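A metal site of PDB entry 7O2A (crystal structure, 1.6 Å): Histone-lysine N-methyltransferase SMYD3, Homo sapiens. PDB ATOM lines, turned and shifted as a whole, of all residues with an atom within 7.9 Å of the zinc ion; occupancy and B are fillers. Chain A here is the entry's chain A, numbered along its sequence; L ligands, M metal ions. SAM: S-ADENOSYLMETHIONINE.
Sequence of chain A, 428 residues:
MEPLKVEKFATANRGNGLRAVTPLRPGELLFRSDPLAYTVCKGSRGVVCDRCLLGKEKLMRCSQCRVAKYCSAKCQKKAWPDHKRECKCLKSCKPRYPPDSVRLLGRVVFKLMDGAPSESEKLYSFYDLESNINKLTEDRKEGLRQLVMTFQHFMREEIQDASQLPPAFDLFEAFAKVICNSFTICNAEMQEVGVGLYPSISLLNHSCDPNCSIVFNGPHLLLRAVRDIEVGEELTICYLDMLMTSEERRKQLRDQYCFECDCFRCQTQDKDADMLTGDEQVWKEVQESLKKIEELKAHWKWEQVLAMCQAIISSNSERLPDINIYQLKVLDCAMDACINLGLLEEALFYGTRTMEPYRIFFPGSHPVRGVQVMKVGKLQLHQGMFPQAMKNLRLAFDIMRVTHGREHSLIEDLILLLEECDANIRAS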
ATOM      1  N   HIS A 206       5.345 -12.531  19.747  1.00  0.00           N
ATOM      2  CA  HIS A 206       4.585 -11.293  19.506  1.00  0.00           C
ATOM      3  C   HIS A 206       4.350 -11.010  18.016  1.00  0.00           C
ATOM      4  O   HIS A 206       5.253 -11.159  17.209  1.00  0.00           O
ATOM      5  CB  HIS A 206       5.348 -10.110  20.076  1.00  0.00           C
ATOM      6  CG  HIS A 206       4.784  -8.765  19.637  1.00  0.00           C
ATOM      7  ND1 HIS A 206       3.689  -8.212  20.229  1.00  0.00           N
ATOM      8  CD2 HIS A 206       5.113  -7.941  18.619  1.00  0.00           C
ATOM      9  CE1 HIS A 206       3.371  -7.096  19.637  1.00  0.00           C
ATOM     10  NE2 HIS A 206       4.242  -6.892  18.676  1.00  0.00           N
ATOM     11  N   SER A 207       3.173 -10.489  17.675  1.00  0.00           N
ATOM     12  CA  SER A 207       2.925  -9.807  16.419  1.00  0.00           C
ATOM     13  C   SER A 207       2.091  -8.577  16.674  1.00  0.00           C
ATOM     14  O   SER A 207       1.178  -8.582  17.510  1.00  0.00           O
ATOM     15  CB  SER A 207       2.173 -10.735  15.452  1.00  0.00           C
ATOM     16  OG  SER A 207       1.759 -10.047  14.315  1.00  0.00           O
ATOM     17  N   CYS A 208       2.333  -7.503  15.872  1.00  0.00           N
ATOM     18  CA  CYS A 208       1.526  -6.304  15.947  1.00  0.00           C
ATOM     19  C   CYS A 208       0.212  -6.524  15.128  1.00  0.00           C
ATOM     20  O   CYS A 208      -0.692  -5.657  15.118  1.00  0.00           O
ATOM     21  CB  CYS A 208       2.301  -5.157  15.323  1.00  0.00           C
ATOM     22  SG  CYS A 208       3.843  -4.791  16.151  1.00  0.00           S
ATOM     23  N   ASP A 209       0.107  -7.673  14.487  1.00  0.00           N
ATOM     24  CA  ASP A 209      -1.149  -8.098  13.816  1.00  0.00           C
ATOM     25  C   ASP A 209      -1.336  -9.620  13.900  1.00  0.00           C
ATOM     26  O   ASP A 209      -1.001 -10.388  12.959  1.00  0.00           O
ATOM     27  CB  ASP A 209      -1.137  -7.646  12.379  1.00  0.00           C
ATOM     28  CG  ASP A 209      -2.369  -8.076  11.599  1.00  0.00           C
ATOM     29  OD1 ASP A 209      -3.407  -8.465  12.172  1.00  0.00           O
ATOM     30  OD2 ASP A 209      -2.307  -7.912  10.354  1.00  0.00           O
ATOM     31  N   SER A 246       3.661   3.062  16.523  1.00  0.00           N
ATOM     32  CA  SER A 246       4.814   2.249  16.256  1.00  0.00           C
ATOM     33  C   SER A 246       6.050   2.675  17.077  1.00  0.00           C
ATOM     34  O   SER A 246       6.832   1.805  17.484  1.00  0.00           O
ATOM     35  CB  SER A 246       5.139   2.210  14.751  1.00  0.00           C
ATOM     36  OG  SER A 246       5.547   3.447  14.235  1.00  0.00           O
ATOM     37  N   ARG A 249       5.393   1.269  20.491  1.00  0.00           N
ATOM     38  CA  ARG A 249       5.603  -0.179  20.513  1.00  0.00           C
ATOM     39  C   ARG A 249       7.108  -0.498  20.475  1.00  0.00           C
ATOM     40  O   ARG A 249       7.592  -1.362  21.146  1.00  0.00           O
ATOM     41  CB  ARG A 249       4.908  -0.908  19.363  1.00  0.00           C
ATOM     42  CG  ARG A 249       3.391  -0.799  19.386  1.00  0.00           C
ATOM     43  CD  ARG A 249       2.739  -1.819  18.477  1.00  0.00           C
ATOM     44  NE  ARG A 249       3.122  -1.744  17.067  1.00  0.00           N
ATOM     45  CZ  ARG A 249       2.637  -0.862  16.186  1.00  0.00           C
ATOM     46  NH1 ARG A 249       1.737   0.107  16.527  1.00  0.00           N
ATOM     47  NH2 ARG A 249       3.059  -0.928  14.935  1.00  0.00           N
ATOM     48  N   ARG A 250       7.875   0.248  19.685  1.00  0.00           N
ATOM     49  CA  ARG A 250       9.306   0.075  19.616  1.00  0.00           C
ATOM     50  C   ARG A 250       9.937   0.218  20.974  1.00  0.00           C
ATOM     51  O   ARG A 250      10.787  -0.578  21.344  1.00  0.00           O
ATOM     52  CB  ARG A 250       9.944   1.069  18.651  1.00  0.00           C
ATOM     53  CG  ARG A 250      11.485   1.099  18.629  1.00  0.00           C
ATOM     54  CD  ARG A 250      12.121   1.973  17.515  1.00  0.00           C
ATOM     55  NE  ARG A 250      11.771   1.425  16.221  1.00  0.00           N
ATOM     56  CZ  ARG A 250      10.870   1.970  15.424  1.00  0.00           C
ATOM     57  NH1 ARG A 250      10.288   3.137  15.699  1.00  0.00           N
ATOM     58  NH2 ARG A 250      10.566   1.339  14.303  1.00  0.00           N
ATOM     59  N   LEU A 253       8.829  -2.825  23.307  1.00  0.00           N
ATOM     60  CA  LEU A 253       9.386  -4.096  22.851  1.00  0.00           C
ATOM     61  C   LEU A 253      10.895  -4.150  23.053  1.00  0.00           C
ATOM     62  O   LEU A 253      11.444  -5.180  23.388  1.00  0.00           O
ATOM     63  CB  LEU A 253       9.000  -4.390  21.375  1.00  0.00           C
ATOM     64  CG  LEU A 253       7.487  -4.575  21.128  1.00  0.00           C
ATOM     65  CD1 LEU A 253       7.208  -4.723  19.646  1.00  0.00           C
ATOM     66  CD2 LEU A 253       6.911  -5.693  22.003  1.00  0.00           C
ATOM     67  N   PHE A 259      13.555  -6.957  21.747  1.00  0.00           N
ATOM     68  CA  PHE A 259      13.610  -7.143  20.328  1.00  0.00           C
ATOM     69  C   PHE A 259      13.073  -5.938  19.560  1.00  0.00           C
ATOM     70  O   PHE A 259      12.418  -5.028  20.153  1.00  0.00           O
ATOM     71  CB  PHE A 259      12.902  -8.456  19.869  1.00  0.00           C
ATOM     72  CG  PHE A 259      11.398  -8.423  19.929  1.00  0.00           C
ATOM     73  CD1 PHE A 259      10.664  -8.110  18.787  1.00  0.00           C
ATOM     74  CD2 PHE A 259      10.730  -8.658  21.108  1.00  0.00           C
ATOM     75  CE1 PHE A 259       9.259  -8.076  18.871  1.00  0.00           C
ATOM     76  CE2 PHE A 259       9.328  -8.603  21.194  1.00  0.00           C
ATOM     77  CZ  PHE A 259       8.607  -8.376  20.079  1.00  0.00           C
ATOM     78  N   GLU A 260      13.467  -5.946  18.288  1.00  0.00           N
ATOM     79  CA  GLU A 260      13.106  -4.971  17.267  1.00  0.00           C
ATOM     80  C   GLU A 260      12.097  -5.647  16.331  1.00  0.00           C
ATOM     81  O   GLU A 260      12.297  -6.729  15.878  1.00  0.00           O
ATOM     82  CB  GLU A 260      14.353  -4.625  16.437  1.00  0.00           C
ATOM     83  CG  GLU A 260      15.628  -4.389  17.271  1.00  0.00           C
ATOM     84  CD  GLU A 260      15.574  -3.220  18.225  1.00  0.00           C
ATOM     85  OE1 GLU A 260      14.628  -2.369  18.118  1.00  0.00           O
ATOM     86  OE2 GLU A 260      16.497  -3.155  19.102  1.00  0.00           O
ATOM     87  N   CYS A 261      11.014  -4.962  16.033  1.00  0.00           N
ATOM     88  CA  CYS A 261      10.005  -5.464  15.087  1.00  0.00           C
ATOM     89  C   CYS A 261      10.112  -4.820  13.725  1.00  0.00           C
ATOM     90  O   CYS A 261      10.120  -3.584  13.630  1.00  0.00           O
ATOM     91  CB  CYS A 261       8.611  -5.178  15.673  1.00  0.00           C
ATOM     92  SG  CYS A 261       7.359  -6.082  14.650  1.00  0.00           S
ATOM     93  N   ASP A 262      10.311  -5.638  12.661  1.00  0.00           N
ATOM     94  CA  ASP A 262      10.254  -5.138  11.269  1.00  0.00           C
ATOM     95  C   ASP A 262       9.034  -5.653  10.516  1.00  0.00           C
ATOM     96  O   ASP A 262       9.102  -5.727   9.307  1.00  0.00           O
ATOM     97  CB  ASP A 262      11.580  -5.437  10.480  1.00  0.00           C
ATOM     98  CG  ASP A 262      11.747  -6.877  10.122  1.00  0.00           C
ATOM     99  OD1 ASP A 262      11.139  -7.754  10.846  1.00  0.00           O
ATOM    100  OD2 ASP A 262      12.536  -7.124   9.123  1.00  0.00           O
ATOM    101  N   CYS A 263       7.917  -5.878  11.210  1.00  0.00           N
ATOM    102  CA  CYS A 263       6.660  -6.181  10.555  1.00  0.00           C
ATOM    103  C   CYS A 263       6.131  -5.094   9.730  1.00  0.00           C
ATOM    104  O   CYS A 263       6.610  -3.980   9.702  1.00  0.00           O
ATOM    105  CB  CYS A 263       5.610  -6.573  11.551  1.00  0.00           C
ATOM    106  SG  CYS A 263       4.664  -5.238  12.343  1.00  0.00           S
ATOM    107  N   PHE A 264       5.193  -5.430   8.845  1.00  0.00           N
ATOM    108  CA  PHE A 264       4.651  -4.443   7.911  1.00  0.00           C
ATOM    109  C   PHE A 264       4.097  -3.186   8.650  1.00  0.00           C
ATOM    110  O   PHE A 264       4.292  -2.082   8.188  1.00  0.00           O
ATOM    111  CB  PHE A 264       3.515  -5.118   7.088  1.00  0.00           C
ATOM    112  CG  PHE A 264       2.639  -4.136   6.362  1.00  0.00           C
ATOM    113  CD1 PHE A 264       3.137  -3.570   5.190  1.00  0.00           C
ATOM    114  CD2 PHE A 264       1.409  -3.736   6.846  1.00  0.00           C
ATOM    115  CE1 PHE A 264       2.421  -2.586   4.496  1.00  0.00           C
ATOM    116  CE2 PHE A 264       0.673  -2.775   6.117  1.00  0.00           C
ATOM    117  CZ  PHE A 264       1.201  -2.224   4.938  1.00  0.00           C
ATOM    118  N   ARG A 265       3.382  -3.405   9.733  1.00  0.00           N
ATOM    119  CA  ARG A 265       2.837  -2.297  10.535  1.00  0.00           C
ATOM    120  C   ARG A 265       3.910  -1.401  11.018  1.00  0.00           C
ATOM    121  O   ARG A 265       3.776  -0.162  10.913  1.00  0.00           O
ATOM    122  CB  ARG A 265       1.969  -2.743  11.714  1.00  0.00           C
ATOM    123  CG  ARG A 265       0.737  -3.507  11.288  1.00  0.00           C
ATOM    124  CD  ARG A 265      -0.293  -3.585  12.387  1.00  0.00           C
ATOM    125  NE  ARG A 265      -0.759  -2.244  12.789  1.00  0.00           N
ATOM    126  CZ  ARG A 265      -0.831  -1.755  14.022  1.00  0.00           C
ATOM    127  NH1 ARG A 265      -0.690  -2.546  15.085  1.00  0.00           N
ATOM    128  NH2 ARG A 265      -1.159  -0.454  14.168  1.00  0.00           N
ATOM    129  N   CYS A 266       4.992  -1.974  11.555  1.00  0.00           N
ATOM    130  CA  CYS A 266       6.070  -1.124  12.097  1.00  0.00           C
ATOM    131  C   CYS A 266       6.877  -0.458  10.963  1.00  0.00           C
ATOM    132  O   CYS A 266       7.208   0.720  11.069  1.00  0.00           O
ATOM    133  CB  CYS A 266       6.966  -1.875  13.062  1.00  0.00           C
ATOM    134  SG  CYS A 266       6.152  -2.436  14.546  1.00  0.00           S
ATOM    135  N   GLN A 267       7.061  -1.158   9.853  1.00  0.00           N
ATOM    136  CA  GLN A 267       7.777  -0.549   8.724  1.00  0.00           C
ATOM    137  C   GLN A 267       7.035   0.576   8.095  1.00  0.00           C
ATOM    138  O   GLN A 267       7.645   1.438   7.421  1.00  0.00           O
ATOM    139  CB  GLN A 267       8.046  -1.588   7.616  1.00  0.00           C
ATOM    140  CG  GLN A 267       9.141  -2.520   8.051  1.00  0.00           C
ATOM    141  CD  GLN A 267       9.947  -3.082   6.893  1.00  0.00           C
ATOM    142  OE1 GLN A 267      10.286  -2.391   5.859  1.00  0.00           O
ATOM    143  NE2 GLN A 267      10.325  -4.336   7.071  1.00  0.00           N
HETATM  144  N   SAM L   1      10.739 -16.718  21.994  1.00  0.00           N
HETATM  145  CA  SAM L   1      10.460 -17.014  23.405  1.00  0.00           C
HETATM  146  C   SAM L   1      11.258 -18.190  23.927  1.00  0.00           C
HETATM  147  O   SAM L   1      12.180 -18.635  23.226  1.00  0.00           O
HETATM  148  OXT SAM L   1      10.986 -18.586  25.069  1.00  0.00           O
HETATM  149  CB  SAM L   1       8.962 -17.179  23.636  1.00  0.00           C
HETATM  150  CG  SAM L   1       8.230 -15.842  23.870  1.00  0.00           C
HETATM  151  SD  SAM L   1       8.656 -14.973  25.316  1.00  0.00           S
HETATM  152  CE  SAM L   1       7.206 -14.624  26.110  1.00  0.00           C
HETATM  153  C5' SAM L   1       9.208 -13.378  24.871  1.00  0.00           C
HETATM  154  C4' SAM L   1      10.511 -13.250  24.115  1.00  0.00           C
HETATM  155  O4' SAM L   1      10.422 -13.872  22.842  1.00  0.00           O
HETATM  156  C3' SAM L   1      10.942 -11.807  23.776  1.00  0.00           C
HETATM  157  O3' SAM L   1      11.474 -11.134  24.931  1.00  0.00           O
HETATM  158  C2' SAM L   1      11.942 -12.020  22.686  1.00  0.00           C
HETATM  159  O2' SAM L   1      13.138 -12.645  23.144  1.00  0.00           O
HETATM  160  C1' SAM L   1      11.147 -13.076  21.887  1.00  0.00           C
HETATM  161  N9  SAM L   1      10.160 -12.494  20.929  1.00  0.00           N
HETATM  162  C8  SAM L   1       8.816 -12.511  21.029  1.00  0.00           C
HETATM  163  N7  SAM L   1       8.250 -12.025  19.930  1.00  0.00           N
HETATM  164  C5  SAM L   1       9.241 -11.766  19.059  1.00  0.00           C
HETATM  165  C6  SAM L   1       9.326 -11.214  17.749  1.00  0.00           C
HETATM  166  N6  SAM L   1       8.233 -10.881  17.055  1.00  0.00           N
HETATM  167  N1  SAM L   1      10.528 -11.019  17.237  1.00  0.00           N
HETATM  168  C2  SAM L   1      11.649 -11.351  17.865  1.00  0.00           C
HETATM  169  N3  SAM L   1      11.684 -11.865  19.092  1.00  0.00           N
HETATM  170  C4  SAM L   1      10.511 -12.063  19.699  1.00  0.00           C
HETATM  171 ZN    ZN M   1       5.556  -4.639  14.442  1.00  0.00          ZN
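N of His 206 sits at hydrogen-bond distance from N7 of the ligand (3.0 Å). A nitrogen (N6) of the ligand sits at hydrogen-bond distance from the backbone carbonyl oxygen (O) of His 206 (3.0 Å).
NH2 of Arg 249 sits close to SG of Cys 266, at 3.5 Å. The backbone NH (N) of Arg 265 lies close to the side-chain sulfur (SG) of Cys 263, at 3.4 Å. The side-chain sulfur of Cys 208 sits close to the guanidinium group of Arg 249, at 3.3 Å. O of Cys 208 sits at hydrogen-bond distance from NH1 of Arg 265 (3.1 Å). N of Cys 208 sits at hydrogen-bond distance from NE2 of His 206, at 3.4 Å.
The nearest printed residue that does not touch the zinc ion is Arg 249 (4.5 Å).
The zinc ion is bound by SG of Cys 266 (2.3 Å), SG of Cys 261 (2.3 Å), SG of Cys 263 (2.4 Å) and SG of Cys 208 (2.4 Å). The zinc ion has four donor atoms within binding distance.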
